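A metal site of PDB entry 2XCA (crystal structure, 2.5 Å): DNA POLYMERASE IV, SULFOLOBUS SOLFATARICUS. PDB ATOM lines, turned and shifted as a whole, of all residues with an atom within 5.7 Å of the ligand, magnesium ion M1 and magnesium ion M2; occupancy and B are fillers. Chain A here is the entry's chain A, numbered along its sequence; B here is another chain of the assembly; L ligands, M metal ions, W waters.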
ATOM      1  N   PHE A  11      12.773  26.971   0.153  1.00  0.00           N
ATOM      2  CA  PHE A  11      13.408  26.123  -0.851  1.00  0.00           C
ATOM      3  C   PHE A  11      12.459  24.997  -1.254  1.00  0.00           C
ATOM      4  O   PHE A  11      11.789  24.391  -0.415  1.00  0.00           O
ATOM      5  CB  PHE A  11      14.708  25.541  -0.266  1.00  0.00           C
ATOM      6  CG  PHE A  11      15.262  24.368  -1.033  1.00  0.00           C
ATOM      7  CD1 PHE A  11      16.082  24.560  -2.153  1.00  0.00           C
ATOM      8  CD2 PHE A  11      15.019  23.056  -0.597  1.00  0.00           C
ATOM      9  CE1 PHE A  11      16.651  23.453  -2.825  1.00  0.00           C
ATOM     10  CE2 PHE A  11      15.576  21.971  -1.268  1.00  0.00           C
ATOM     11  CZ  PHE A  11      16.404  22.162  -2.383  1.00  0.00           C
ATOM     12  N   ASP A  13      12.072  21.381  -3.681  1.00  0.00           N
ATOM     13  CA  ASP A  13      12.759  20.293  -4.359  1.00  0.00           C
ATOM     14  C   ASP A  13      11.729  19.226  -4.779  1.00  0.00           C
ATOM     15  O   ASP A  13      11.008  18.713  -3.932  1.00  0.00           O
ATOM     16  CB  ASP A  13      13.792  19.692  -3.429  1.00  0.00           C
ATOM     17  CG  ASP A  13      14.753  18.774  -4.160  1.00  0.00           C
ATOM     18  OD1 ASP A  13      15.721  19.290  -4.734  1.00  0.00           O
ATOM     19  OD2 ASP A  13      14.517  17.555  -4.156  1.00  0.00           O
ATOM     20  N   PHE A  14      11.676  18.891  -6.070  1.00  0.00           N
ATOM     21  CA  PHE A  14      10.707  17.906  -6.555  1.00  0.00           C
ATOM     22  C   PHE A  14      11.032  16.484  -6.065  1.00  0.00           C
ATOM     23  O   PHE A  14      12.166  16.073  -6.072  1.00  0.00           O
ATOM     24  CB  PHE A  14      10.643  17.911  -8.087  1.00  0.00           C
ATOM     25  CG  PHE A  14      10.631  19.288  -8.681  1.00  0.00           C
ATOM     26  CD1 PHE A  14      10.293  20.393  -7.908  1.00  0.00           C
ATOM     27  CD2 PHE A  14      11.001  19.475 -10.002  1.00  0.00           C
ATOM     28  CE1 PHE A  14      10.324  21.685  -8.458  1.00  0.00           C
ATOM     29  CE2 PHE A  14      11.040  20.738 -10.563  1.00  0.00           C
ATOM     30  CZ  PHE A  14      10.702  21.871  -9.791  1.00  0.00           C
ATOM     31  N   ASP A  15      10.035  15.709  -5.660  1.00  0.00           N
ATOM     32  CA  ASP A  15      10.325  14.381  -5.169  1.00  0.00           C
ATOM     33  C   ASP A  15      10.710  13.379  -6.262  1.00  0.00           C
ATOM     34  O   ASP A  15      10.102  13.373  -7.330  1.00  0.00           O
ATOM     35  CB  ASP A  15       9.147  13.870  -4.349  1.00  0.00           C
ATOM     36  CG  ASP A  15       8.916  14.710  -3.104  1.00  0.00           C
ATOM     37  OD1 ASP A  15       9.883  15.322  -2.596  1.00  0.00           O
ATOM     38  OD2 ASP A  15       7.777  14.755  -2.610  1.00  0.00           O
ATOM     39  N   TYR A  16      11.717  12.546  -5.990  1.00  0.00           N
ATOM     40  CA  TYR A  16      12.203  11.532  -6.958  1.00  0.00           C
ATOM     41  C   TYR A  16      11.803  11.922  -8.365  1.00  0.00           C
ATOM     42  O   TYR A  16      11.263  11.132  -9.134  1.00  0.00           O
ATOM     43  CB  TYR A  16      11.654  10.132  -6.573  1.00  0.00           C
ATOM     44  CG  TYR A  16      10.136   9.993  -6.544  1.00  0.00           C
ATOM     45  CD1 TYR A  16       9.449   9.436  -7.636  1.00  0.00           C
ATOM     46  CD2 TYR A  16       9.395  10.408  -5.436  1.00  0.00           C
ATOM     47  CE1 TYR A  16       8.077   9.294  -7.620  1.00  0.00           C
ATOM     48  CE2 TYR A  16       8.002  10.259  -5.424  1.00  0.00           C
ATOM     49  CZ  TYR A  16       7.351   9.709  -6.520  1.00  0.00           C
ATOM     50  OH  TYR A  16       5.965   9.601  -6.539  1.00  0.00           O
ATOM     51  N   PHE A  17      12.137  13.165  -8.697  1.00  0.00           N
ATOM     52  CA  PHE A  17      11.801  13.821  -9.955  1.00  0.00           C
ATOM     53  C   PHE A  17      11.723  13.083 -11.284  1.00  0.00           C
ATOM     54  O   PHE A  17      10.636  13.031 -11.860  1.00  0.00           O
ATOM     55  CB  PHE A  17      12.651  15.087 -10.121  1.00  0.00           C
ATOM     56  CG  PHE A  17      12.146  16.013 -11.202  1.00  0.00           C
ATOM     57  CD1 PHE A  17      10.802  16.363 -11.272  1.00  0.00           C
ATOM     58  CD2 PHE A  17      13.011  16.506 -12.160  1.00  0.00           C
ATOM     59  CE1 PHE A  17      10.325  17.192 -12.283  1.00  0.00           C
ATOM     60  CE2 PHE A  17      12.554  17.340 -13.185  1.00  0.00           C
ATOM     61  CZ  PHE A  17      11.203  17.677 -13.243  1.00  0.00           C
ATOM     62  N   TYR A  18      12.821  12.537 -11.789  1.00  0.00           N
ATOM     63  CA  TYR A  18      12.763  11.855 -13.093  1.00  0.00           C
ATOM     64  C   TYR A  18      11.807  10.693 -13.082  1.00  0.00           C
ATOM     65  O   TYR A  18      11.096  10.438 -14.053  1.00  0.00           O
ATOM     66  CB  TYR A  18      14.146  11.328 -13.491  1.00  0.00           C
ATOM     67  CG  TYR A  18      15.138  12.371 -13.926  1.00  0.00           C
ATOM     68  CD1 TYR A  18      14.921  13.713 -13.664  1.00  0.00           C
ATOM     69  CD2 TYR A  18      16.327  12.004 -14.548  1.00  0.00           C
ATOM     70  CE1 TYR A  18      15.864  14.682 -14.034  1.00  0.00           C
ATOM     71  CE2 TYR A  18      17.266  12.937 -14.911  1.00  0.00           C
ATOM     72  CZ  TYR A  18      17.041  14.279 -14.655  1.00  0.00           C
ATOM     73  OH  TYR A  18      17.964  15.213 -15.010  1.00  0.00           O
ATOM     74  N   ALA A  19      11.782   9.955 -11.980  1.00  0.00           N
ATOM     75  CA  ALA A  19      10.910   8.808 -11.856  1.00  0.00           C
ATOM     76  C   ALA A  19       9.460   9.292 -11.780  1.00  0.00           C
ATOM     77  O   ALA A  19       8.582   8.786 -12.503  1.00  0.00           O
ATOM     78  CB  ALA A  19      11.283   8.002 -10.644  1.00  0.00           C
ATOM     79  N   VAL A  38      20.517   5.378 -17.121  1.00  0.00           N
ATOM     80  CA  VAL A  38      21.338   5.968 -18.142  1.00  0.00           C
ATOM     81  C   VAL A  38      22.171   4.804 -18.692  1.00  0.00           C
ATOM     82  O   VAL A  38      23.209   4.446 -18.111  1.00  0.00           O
ATOM     83  CB  VAL A  38      22.256   7.064 -17.567  1.00  0.00           C
ATOM     84  CG1 VAL A  38      23.234   7.536 -18.640  1.00  0.00           C
ATOM     85  CG2 VAL A  38      21.443   8.199 -17.053  1.00  0.00           C
ATOM     86  N   VAL A  49      22.152   4.365 -12.494  1.00  0.00           N
ATOM     87  CA  VAL A  49      20.805   4.789 -12.218  1.00  0.00           C
ATOM     88  C   VAL A  49      20.751   6.296 -12.017  1.00  0.00           C
ATOM     89  O   VAL A  49      21.464   6.830 -11.170  1.00  0.00           O
ATOM     90  CB  VAL A  49      20.272   4.108 -10.937  1.00  0.00           C
ATOM     91  CG1 VAL A  49      18.955   4.755 -10.531  1.00  0.00           C
ATOM     92  CG2 VAL A  49      20.102   2.605 -11.170  1.00  0.00           C
ATOM     93  N   ALA A  50      19.919   6.989 -12.794  1.00  0.00           N
ATOM     94  CA  ALA A  50      19.786   8.454 -12.637  1.00  0.00           C
ATOM     95  C   ALA A  50      19.060   8.734 -11.336  1.00  0.00           C
ATOM     96  O   ALA A  50      19.471   9.612 -10.563  1.00  0.00           O
ATOM     97  CB  ALA A  50      19.021   9.058 -13.789  1.00  0.00           C
ATOM     98  N   THR A  51      17.987   7.991 -11.099  1.00  0.00           N
ATOM     99  CA  THR A  51      17.178   8.050  -9.877  1.00  0.00           C
ATOM    100  C   THR A  51      16.105   6.953  -9.863  1.00  0.00           C
ATOM    101  O   THR A  51      15.867   6.292 -10.855  1.00  0.00           O
ATOM    102  CB  THR A  51      16.451   9.393  -9.690  1.00  0.00           C
ATOM    103  OG1 THR A  51      16.001   9.506  -8.329  1.00  0.00           O
ATOM    104  CG2 THR A  51      15.214   9.496 -10.628  1.00  0.00           C
ATOM    105  N   ALA A  52      15.444   6.788  -8.718  1.00  0.00           N
ATOM    106  CA  ALA A  52      14.398   5.787  -8.570  1.00  0.00           C
ATOM    107  C   ALA A  52      13.350   6.317  -7.611  1.00  0.00           C
ATOM    108  O   ALA A  52      13.692   7.094  -6.719  1.00  0.00           O
ATOM    109  CB  ALA A  52      14.971   4.505  -8.007  1.00  0.00           C
ATOM    110  N   TYR A  54      10.635   6.195  -4.483  1.00  0.00           N
ATOM    111  CA  TYR A  54      10.882   5.721  -3.113  1.00  0.00           C
ATOM    112  C   TYR A  54      10.637   4.240  -2.875  1.00  0.00           C
ATOM    113  O   TYR A  54      11.262   3.645  -2.000  1.00  0.00           O
ATOM    114  CB  TYR A  54      10.096   6.580  -2.106  1.00  0.00           C
ATOM    115  CG  TYR A  54      10.736   7.946  -1.908  1.00  0.00           C
ATOM    116  CD1 TYR A  54      10.749   8.885  -2.927  1.00  0.00           C
ATOM    117  CD2 TYR A  54      11.362   8.252  -0.710  1.00  0.00           C
ATOM    118  CE1 TYR A  54      11.371  10.116  -2.758  1.00  0.00           C
ATOM    119  CE2 TYR A  54      11.994   9.483  -0.519  1.00  0.00           C
ATOM    120  CZ  TYR A  54      11.993  10.415  -1.554  1.00  0.00           C
ATOM    121  OH  TYR A  54      12.578  11.654  -1.382  1.00  0.00           O
ATOM    122  N   ARG A  57      13.856   2.832  -3.599  1.00  0.00           N
ATOM    123  CA  ARG A  57      14.952   3.254  -2.715  1.00  0.00           C
ATOM    124  C   ARG A  57      14.966   2.500  -1.402  1.00  0.00           C
ATOM    125  O   ARG A  57      15.975   2.501  -0.690  1.00  0.00           O
ATOM    126  CB  ARG A  57      14.876   4.750  -2.396  1.00  0.00           C
ATOM    127  CG  ARG A  57      15.161   5.665  -3.567  1.00  0.00           C
ATOM    128  CD  ARG A  57      15.181   7.114  -3.134  1.00  0.00           C
ATOM    129  NE  ARG A  57      15.004   7.989  -4.284  1.00  0.00           N
ATOM    130  CZ  ARG A  57      15.010   9.328  -4.229  1.00  0.00           C
ATOM    131  NH1 ARG A  57      15.202   9.932  -3.057  1.00  0.00           N
ATOM    132  NH2 ARG A  57      14.821  10.042  -5.339  1.00  0.00           N
ATOM    133  N   ALA A  63      20.262   6.660  -7.185  1.00  0.00           N
ATOM    134  CA  ALA A  63      21.144   7.380  -8.110  1.00  0.00           C
ATOM    135  C   ALA A  63      22.616   7.062  -7.821  1.00  0.00           C
ATOM    136  O   ALA A  63      23.054   7.066  -6.678  1.00  0.00           O
ATOM    137  CB  ALA A  63      20.903   8.888  -7.985  1.00  0.00           C
ATOM    138  N   GLY A  64      23.361   6.769  -8.874  1.00  0.00           N
ATOM    139  CA  GLY A  64      24.771   6.477  -8.719  1.00  0.00           C
ATOM    140  C   GLY A  64      25.186   5.027  -8.885  1.00  0.00           C
ATOM    141  O   GLY A  64      26.223   4.762  -9.502  1.00  0.00           O
ATOM    142  N   MET A  82      16.465   7.136 -19.235  1.00  0.00           N
ATOM    143  CA  MET A  82      16.331   8.550 -18.896  1.00  0.00           C
ATOM    144  C   MET A  82      15.972   9.419 -20.111  1.00  0.00           C
ATOM    145  O   MET A  82      16.655   9.390 -21.136  1.00  0.00           O
ATOM    146  CB  MET A  82      17.638   9.066 -18.278  1.00  0.00           C
ATOM    147  CG  MET A  82      17.605  10.548 -17.933  1.00  0.00           C
ATOM    148  SD  MET A  82      19.195  11.133 -17.424  1.00  0.00           S
ATOM    149  CE  MET A  82      20.015  11.346 -19.026  1.00  0.00           C
ATOM    150  N   SER A 109      19.194  23.677  -9.576  1.00  0.00           N
ATOM    151  CA  SER A 109      19.368  22.401 -10.265  1.00  0.00           C
ATOM    152  C   SER A 109      18.143  22.187 -11.125  1.00  0.00           C
ATOM    153  O   SER A 109      17.285  23.065 -11.215  1.00  0.00           O
ATOM    154  CB  SER A 109      19.464  21.247  -9.255  1.00  0.00           C
ATOM    155  OG  SER A 109      18.177  20.775  -8.867  1.00  0.00           O
ATOM    156  N   ILE A 110      18.062  21.031 -11.770  1.00  0.00           N
ATOM    157  CA  ILE A 110      16.911  20.745 -12.618  1.00  0.00           C
ATOM    158  C   ILE A 110      15.645  20.554 -11.804  1.00  0.00           C
ATOM    159  O   ILE A 110      14.550  20.488 -12.368  1.00  0.00           O
ATOM    160  CB  ILE A 110      17.146  19.506 -13.452  1.00  0.00           C
ATOM    161  CG1 ILE A 110      16.068  19.396 -14.526  1.00  0.00           C
ATOM    162  CG2 ILE A 110      17.132  18.281 -12.552  1.00  0.00           C
ATOM    163  CD1 ILE A 110      16.440  18.491 -15.696  1.00  0.00           C
ATOM    164  N   ASP A 111      15.745  20.471 -10.477  1.00  0.00           N
ATOM    165  CA  ASP A 111      14.504  20.270  -9.706  1.00  0.00           C
ATOM    166  C   ASP A 111      14.433  20.983  -8.380  1.00  0.00           C
ATOM    167  O   ASP A 111      13.689  20.550  -7.492  1.00  0.00           O
ATOM    168  CB  ASP A 111      14.257  18.775  -9.485  1.00  0.00           C
ATOM    169  CG  ASP A 111      15.085  18.247  -8.341  1.00  0.00           C
ATOM    170  OD1 ASP A 111      16.270  18.630  -8.253  1.00  0.00           O
ATOM    171  OD2 ASP A 111      14.549  17.446  -7.556  1.00  0.00           O
ATOM    172  N   GLU A 112      15.190  22.070  -8.225  1.00  0.00           N
ATOM    173  CA  GLU A 112      15.138  22.808  -6.970  1.00  0.00           C
ATOM    174  C   GLU A 112      15.398  24.305  -7.135  1.00  0.00           C
ATOM    175  O   GLU A 112      16.138  24.746  -8.016  1.00  0.00           O
ATOM    176  CB  GLU A 112      16.098  22.211  -5.935  1.00  0.00           C
ATOM    177  CG  GLU A 112      17.548  22.220  -6.349  1.00  0.00           C
ATOM    178  CD  GLU A 112      18.373  21.165  -5.602  1.00  0.00           C
ATOM    179  OE1 GLU A 112      18.843  21.401  -4.474  1.00  0.00           O
ATOM    180  OE2 GLU A 112      18.530  20.077  -6.160  1.00  0.00           O
ATOM    181  N   LYS A 158      17.470  24.286   2.685  1.00  0.00           N
ATOM    182  CA  LYS A 158      17.791  23.029   2.023  1.00  0.00           C
ATOM    183  C   LYS A 158      17.732  21.879   3.041  1.00  0.00           C
ATOM    184  O   LYS A 158      17.144  20.836   2.794  1.00  0.00           O
ATOM    185  CB  LYS A 158      19.187  23.125   1.403  1.00  0.00           C
ATOM    186  CG  LYS A 158      19.759  21.830   0.846  1.00  0.00           C
ATOM    187  CD  LYS A 158      18.998  21.343  -0.340  1.00  0.00           C
ATOM    188  CE  LYS A 158      19.568  20.029  -0.872  1.00  0.00           C
ATOM    189  NZ  LYS A 158      18.776  19.486  -2.025  1.00  0.00           N
ATOM    190  N   LYS A 165      11.661  15.211   3.448  1.00  0.00           N
ATOM    191  CA  LYS A 165      11.434  14.388   2.257  1.00  0.00           C
ATOM    192  C   LYS A 165      10.752  13.069   2.653  1.00  0.00           C
ATOM    193  O   LYS A 165      11.127  12.468   3.661  1.00  0.00           O
ATOM    194  CB  LYS A 165      12.766  14.086   1.567  1.00  0.00           C
ATOM    195  CG  LYS A 165      13.322  15.181   0.667  1.00  0.00           C
ATOM    196  CD  LYS A 165      12.674  15.146  -0.710  1.00  0.00           C
ATOM    197  CE  LYS A 165      13.192  16.262  -1.625  1.00  0.00           C
ATOM    198  NZ  LYS A 165      12.585  16.212  -2.994  1.00  0.00           N
ATOM    199  N   PRO A 166       9.755  12.605   1.877  1.00  0.00           N
ATOM    200  CA  PRO A 166       9.204  13.203   0.653  1.00  0.00           C
ATOM    201  C   PRO A 166       7.857  13.860   0.911  1.00  0.00           C
ATOM    202  O   PRO A 166       7.286  13.726   2.000  1.00  0.00           O
ATOM    203  CB  PRO A 166       9.088  12.010  -0.272  1.00  0.00           C
ATOM    204  CG  PRO A 166       8.614  10.951   0.666  1.00  0.00           C
ATOM    205  CD  PRO A 166       9.452  11.162   1.916  1.00  0.00           C
ATOM    206  P    DC B   4      30.090   5.241 -15.827  1.00  0.00           P
ATOM    207  OP1  DC B   4      30.843   4.364 -16.778  1.00  0.00           O
ATOM    208  OP2  DC B   4      30.810   6.146 -14.910  1.00  0.00           O
ATOM    209  O5'  DC B   4      28.970   6.033 -16.603  1.00  0.00           O
ATOM    210  C5'  DC B   4      27.940   5.264 -17.223  1.00  0.00           C
ATOM    211  C4'  DC B   4      26.770   6.159 -17.632  1.00  0.00           C
ATOM    212  O4'  DC B   4      26.068   6.674 -16.473  1.00  0.00           O
ATOM    213  C3'  DC B   4      27.319   7.408 -18.338  1.00  0.00           C
ATOM    214  O3'  DC B   4      26.430   7.742 -19.379  1.00  0.00           O
ATOM    215  C2'  DC B   4      27.349   8.466 -17.245  1.00  0.00           C
ATOM    216  C1'  DC B   4      26.154   8.089 -16.416  1.00  0.00           C
ATOM    217  N1   DC B   4      26.228   8.455 -15.000  1.00  0.00           N
ATOM    218  C2   DC B   4      25.238   9.269 -14.461  1.00  0.00           C
ATOM    219  O2   DC B   4      24.367   9.703 -15.209  1.00  0.00           O
ATOM    220  N3   DC B   4      25.239   9.556 -13.140  1.00  0.00           N
ATOM    221  C4   DC B   4      26.203   9.037 -12.351  1.00  0.00           C
ATOM    222  N4   DC B   4      26.132   9.289 -11.047  1.00  0.00           N
ATOM    223  C5   DC B   4      27.256   8.243 -12.880  1.00  0.00           C
ATOM    224  C6   DC B   4      27.239   7.985 -14.194  1.00  0.00           C
ATOM    225  P   8OG B   5      26.961   8.593 -20.635  1.00  0.00           P
ATOM    226  OP1 8OG B   5      26.077   8.363 -21.805  1.00  0.00           O
ATOM    227  OP2 8OG B   5      28.414   8.340 -20.775  1.00  0.00           O
ATOM    228  O5' 8OG B   5      26.742  10.097 -20.169  1.00  0.00           O
ATOM    229  C5' 8OG B   5      25.406  10.521 -19.871  1.00  0.00           C
ATOM    230  C4' 8OG B   5      25.435  11.654 -18.855  1.00  0.00           C
ATOM    231  O4' 8OG B   5      26.093  11.274 -17.635  1.00  0.00           O
ATOM    232  C3' 8OG B   5      26.230  12.870 -19.328  1.00  0.00           C
ATOM    233  O3' 8OG B   5      25.319  13.773 -20.005  1.00  0.00           O
ATOM    234  C2' 8OG B   5      26.778  13.470 -18.033  1.00  0.00           C
ATOM    235  C1' 8OG B   5      26.221  12.530 -16.951  1.00  0.00           C
ATOM    236  N9  8OG B   5      27.059  12.365 -15.743  1.00  0.00           N
ATOM    237  C8  8OG B   5      28.267  11.820 -15.678  1.00  0.00           C
ATOM    238  N7  8OG B   5      28.658  11.637 -14.415  1.00  0.00           N
ATOM    239  C5  8OG B   5      27.676  12.110 -13.670  1.00  0.00           C
ATOM    240  C6  8OG B   5      27.551  12.196 -12.292  1.00  0.00           C
ATOM    241  O6  8OG B   5      28.392  11.749 -11.511  1.00  0.00           O
ATOM    242  N1  8OG B   5      26.383  12.778 -11.805  1.00  0.00           N
ATOM    243  C2  8OG B   5      25.389  13.232 -12.682  1.00  0.00           C
ATOM    244  N2  8OG B   5      24.297  13.791 -12.207  1.00  0.00           N
ATOM    245  N3  8OG B   5      25.538  13.139 -14.022  1.00  0.00           N
ATOM    246  C4  8OG B   5      26.647  12.594 -14.487  1.00  0.00           C
ATOM    247  O8  8OG B   5      28.897  11.537 -16.691  1.00  0.00           O
HETATM  248  P1  LIG L   1      14.483  13.401  -3.957  1.00  0.00           P
HETATM  249  O1  LIG L   1      15.328  12.769  -2.742  1.00  0.00           O
HETATM  250  O2  LIG L   1      15.142  14.844  -4.232  1.00  0.00           O
HETATM  251  O3  LIG L   1      13.038  13.481  -3.633  1.00  0.00           O
HETATM  252  O4  LIG L   1      14.795  12.493  -5.243  1.00  0.00           O
HETATM  253  P2  LIG L   1      15.370  13.092  -6.618  1.00  0.00           P
HETATM  254  O5  LIG L   1      15.378  11.988  -7.597  1.00  0.00           O
HETATM  255  O6  LIG L   1      14.624  14.321  -6.960  1.00  0.00           O
HETATM  256  O7  LIG L   1      16.888  13.449  -6.206  1.00  0.00           O
HETATM  257  P3  LIG L   1      17.473  14.947  -6.152  1.00  0.00           P
HETATM  258  O8  LIG L   1      16.347  16.094  -6.137  1.00  0.00           O
HETATM  259  O9  LIG L   1      18.824  15.205  -5.612  1.00  0.00           O
HETATM  260  O10 LIG L   1      17.801  15.014  -7.721  1.00  0.00           O
HETATM  261  C1  LIG L   1      16.812  15.430  -8.667  1.00  0.00           C
HETATM  262  C2  LIG L   1      17.056  14.776 -10.035  1.00  0.00           C
HETATM  263  O11 LIG L   1      18.362  15.039 -10.576  1.00  0.00           O
HETATM  264  C3  LIG L   1      16.978  13.251  -9.985  1.00  0.00           C
HETATM  265  O12 LIG L   1      15.613  12.847  -9.963  1.00  0.00           O
HETATM  266  C4  LIG L   1      17.556  12.958 -11.371  1.00  0.00           C
HETATM  267  C5  LIG L   1      18.768  13.911 -11.365  1.00  0.00           C
HETATM  268  N1  LIG L   1      19.925  13.263 -10.713  1.00  0.00           N
HETATM  269  C6  LIG L   1      20.267  13.323  -9.423  1.00  0.00           C
HETATM  270  N2  LIG L   1      21.378  12.628  -9.212  1.00  0.00           N
HETATM  271  C7  LIG L   1      21.775  12.133 -10.384  1.00  0.00           C
HETATM  272  C8  LIG L   1      22.837  11.322 -10.767  1.00  0.00           C
HETATM  273  O13 LIG L   1      23.691  10.933  -9.948  1.00  0.00           O
HETATM  274  N3  LIG L   1      22.946  10.947 -12.119  1.00  0.00           N
HETATM  275  C9  LIG L   1      21.985  11.378 -13.033  1.00  0.00           C
HETATM  276  N4  LIG L   1      22.056  10.985 -14.299  1.00  0.00           N
HETATM  277  N5  LIG L   1      20.966  12.160 -12.623  1.00  0.00           N
HETATM  278  C10 LIG L   1      20.839  12.526 -11.340  1.00  0.00           C
HETATM  279 MG    MG M   1      16.949  18.462  -6.287  1.00  0.00          MG
HETATM  280 MG    MG M   2      14.159  16.022  -5.745  1.00  0.00          MG
HETATM  281  O   HOH W   1      26.554  12.368  -8.561  1.00  0.00           O
HETATM  282  O   HOH W   2      16.305  16.126  -2.479  1.00  0.00           O
HETATM  283  O   HOH W   3      19.839  17.574 -10.244  1.00  0.00           O
HETATM  284  O   HOH W   4      24.830  10.494  -7.061  1.00  0.00           O
HETATM  285  O   HOH W   5      18.001  17.818  -4.413  1.00  0.00           O
HETATM  286  O   HOH W   6      18.832  17.770  -7.395  1.00  0.00           O
HETATM  287  O   HOH W   7      20.409  13.974 -15.052  1.00  0.00           O
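Merely in contact with magnesium ion M1: Ser 109 (3.7 Å). Of the 27 residues printed, 4 come within 4 Å of magnesium ion M1. Along chain A the residues within 4 Å of magnesium ion M1 span positions 13 to 112. The nearest printed residue that does not touch magnesium ion M1 is Lys 158 (4.7 Å).
Water W5 bridges an oxygen (O9) of the ligand (3.0 Å) and the side-chain amino group (NZ) of Lys 158 (3.0 Å). Water W6 lies within hydrogen-bond range of an oxygen (O10) of the ligand and the side-chain hydroxyl of Ser 109. Water W7 lies within hydrogen-bond range of OH of Tyr 18 (2.7 Å) and N5 of the ligand (3.1 Å). Water W1 bridges N1 of 8OG 5 of chain B (3.3 Å) and O13 of the ligand (3.5 Å).
The backbone carbonyl oxygen (O) of Phe 14 lies close to the side-chain amino group (NZ) of Lys 165 (3.1 Å). The backbone NH (N) of Asp 111 is in hydrogen-bond range of the side-chain hydroxyl (OG) of Ser 109, 2.9 Å away. NZ of Lys 165 lies within hydrogen-bond range of O of Asp 13 (3.1 Å). The backbone NH (N) of Glu 112 sits close to the side-chain hydroxyl (OG) of Ser 109. The side-chain carboxylate (OE1) of Glu 112 lies within salt-bridge range of the side-chain amino group (NZ) of Lys 158 (3.1 Å). The guanidinium group of Arg 57 sits at hydrogen-bond distance from the side-chain hydroxyl of Thr 51 (3.3 Å). O of Ala 52 lies within hydrogen-bond range of NE of Arg 57 (2.9 Å). The side-chain amino group (NZ) of Lys 165 lies within salt-bridge range of the side-chain carboxylate (OD1) of Asp 15, 2.9 Å away.
CA of Asp 15 touches O3 of the ligand (3.2 Å). CG2 of Val 38 touches N4 of the ligand (3.97 Å). Ala 50 touches the ligand (O to C10, 3.3 Å). CB of Ala 63 touches N2 of the ligand, at 3.96 Å. Ile 110 touches the ligand. Hydrophobic or aromatic side chains within 4 Å of the ligand: Phe 17, Tyr 18, Val 38, Ala 50, Tyr 54, Ala 63 and Ile 110. Within 4 Å of the ligand: Asp 13, Phe 14, Asp 15, Tyr 16, Phe 17, Tyr 18, Val 38, Ala 50, Thr 51, Tyr 54, Arg 57, Ala 63, Ile 110, Asp 111, Lys 165, DC 4 of chain B and 8OG 5 of chain B.
Merely in contact with magnesium ion M2: Lys 165. Within 4 Å of magnesium ion M2: Asp 13, Phe 14, Asp 111 and Lys 165. The nearest printed residue that does not touch magnesium ion M2 is Asp 15 (4.1 Å).
The side-chain carboxylate (OD1) of Asp 111 is bound to magnesium ion M1, at 2.1 Å. Magnesium ion M1 is bound by the side-chain carboxylate (OD1) of Asp 13, at 2.1 Å. Magnesium ion M1 is bound by water W5 (2.2 Å). Magnesium ion M1 is bound by the side-chain carboxylate (OE2) of Glu 112, at 2.3 Å. Water W6 binds magnesium ion M1 (2.3 Å). An oxygen (O8) of the ligand is bound to magnesium ion M1, at 2.4 Å. Magnesium ion M1 has six donor atoms within binding distance.
O1 of the ligand lies within salt-bridge range of NH1 of Arg 57. The side-chain hydroxyl (OG1) of Thr 51 sits at hydrogen-bond distance from an oxygen (O5) of the ligand, at 2.7 Å. O2 of DC 4 of chain B is in hydrogen-bond range of N4 of the ligand. An oxygen (O3) of the ligand is in salt-bridge range of the side-chain amino group (NZ) of Lys 165 (2.8 Å). The backbone NH (N) of Tyr 16 sits at hydrogen-bond distance from an oxygen (O3) of the ligand. OH of Tyr 54 is in hydrogen-bond range of O3 of the ligand. N2 of 8OG 5 of chain B sits at hydrogen-bond distance from N3 of the ligand. The backbone NH (N) of Phe 17 sits close to an oxygen (O6) of the ligand (3.2 Å). N of Tyr 18 is in hydrogen-bond range of O12 of the ligand, at 3.4 Å.
O of Phe 14 is bound to magnesium ion M2 (2.0 Å). O6 of the ligand binds magnesium ion M2 (2.1 Å). O2 of the ligand binds magnesium ion M2 (2.2 Å). O8 of the ligand is bound to magnesium ion M2, 2.2 Å away. Magnesium ion M2 is bound by OD2 of Asp 13 (2.2 Å). Magnesium ion M2 is bound by the side-chain carboxylate (OD2) of Asp 111, at 2.3 Å. Magnesium ion M2 has six donor atoms within binding distance.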
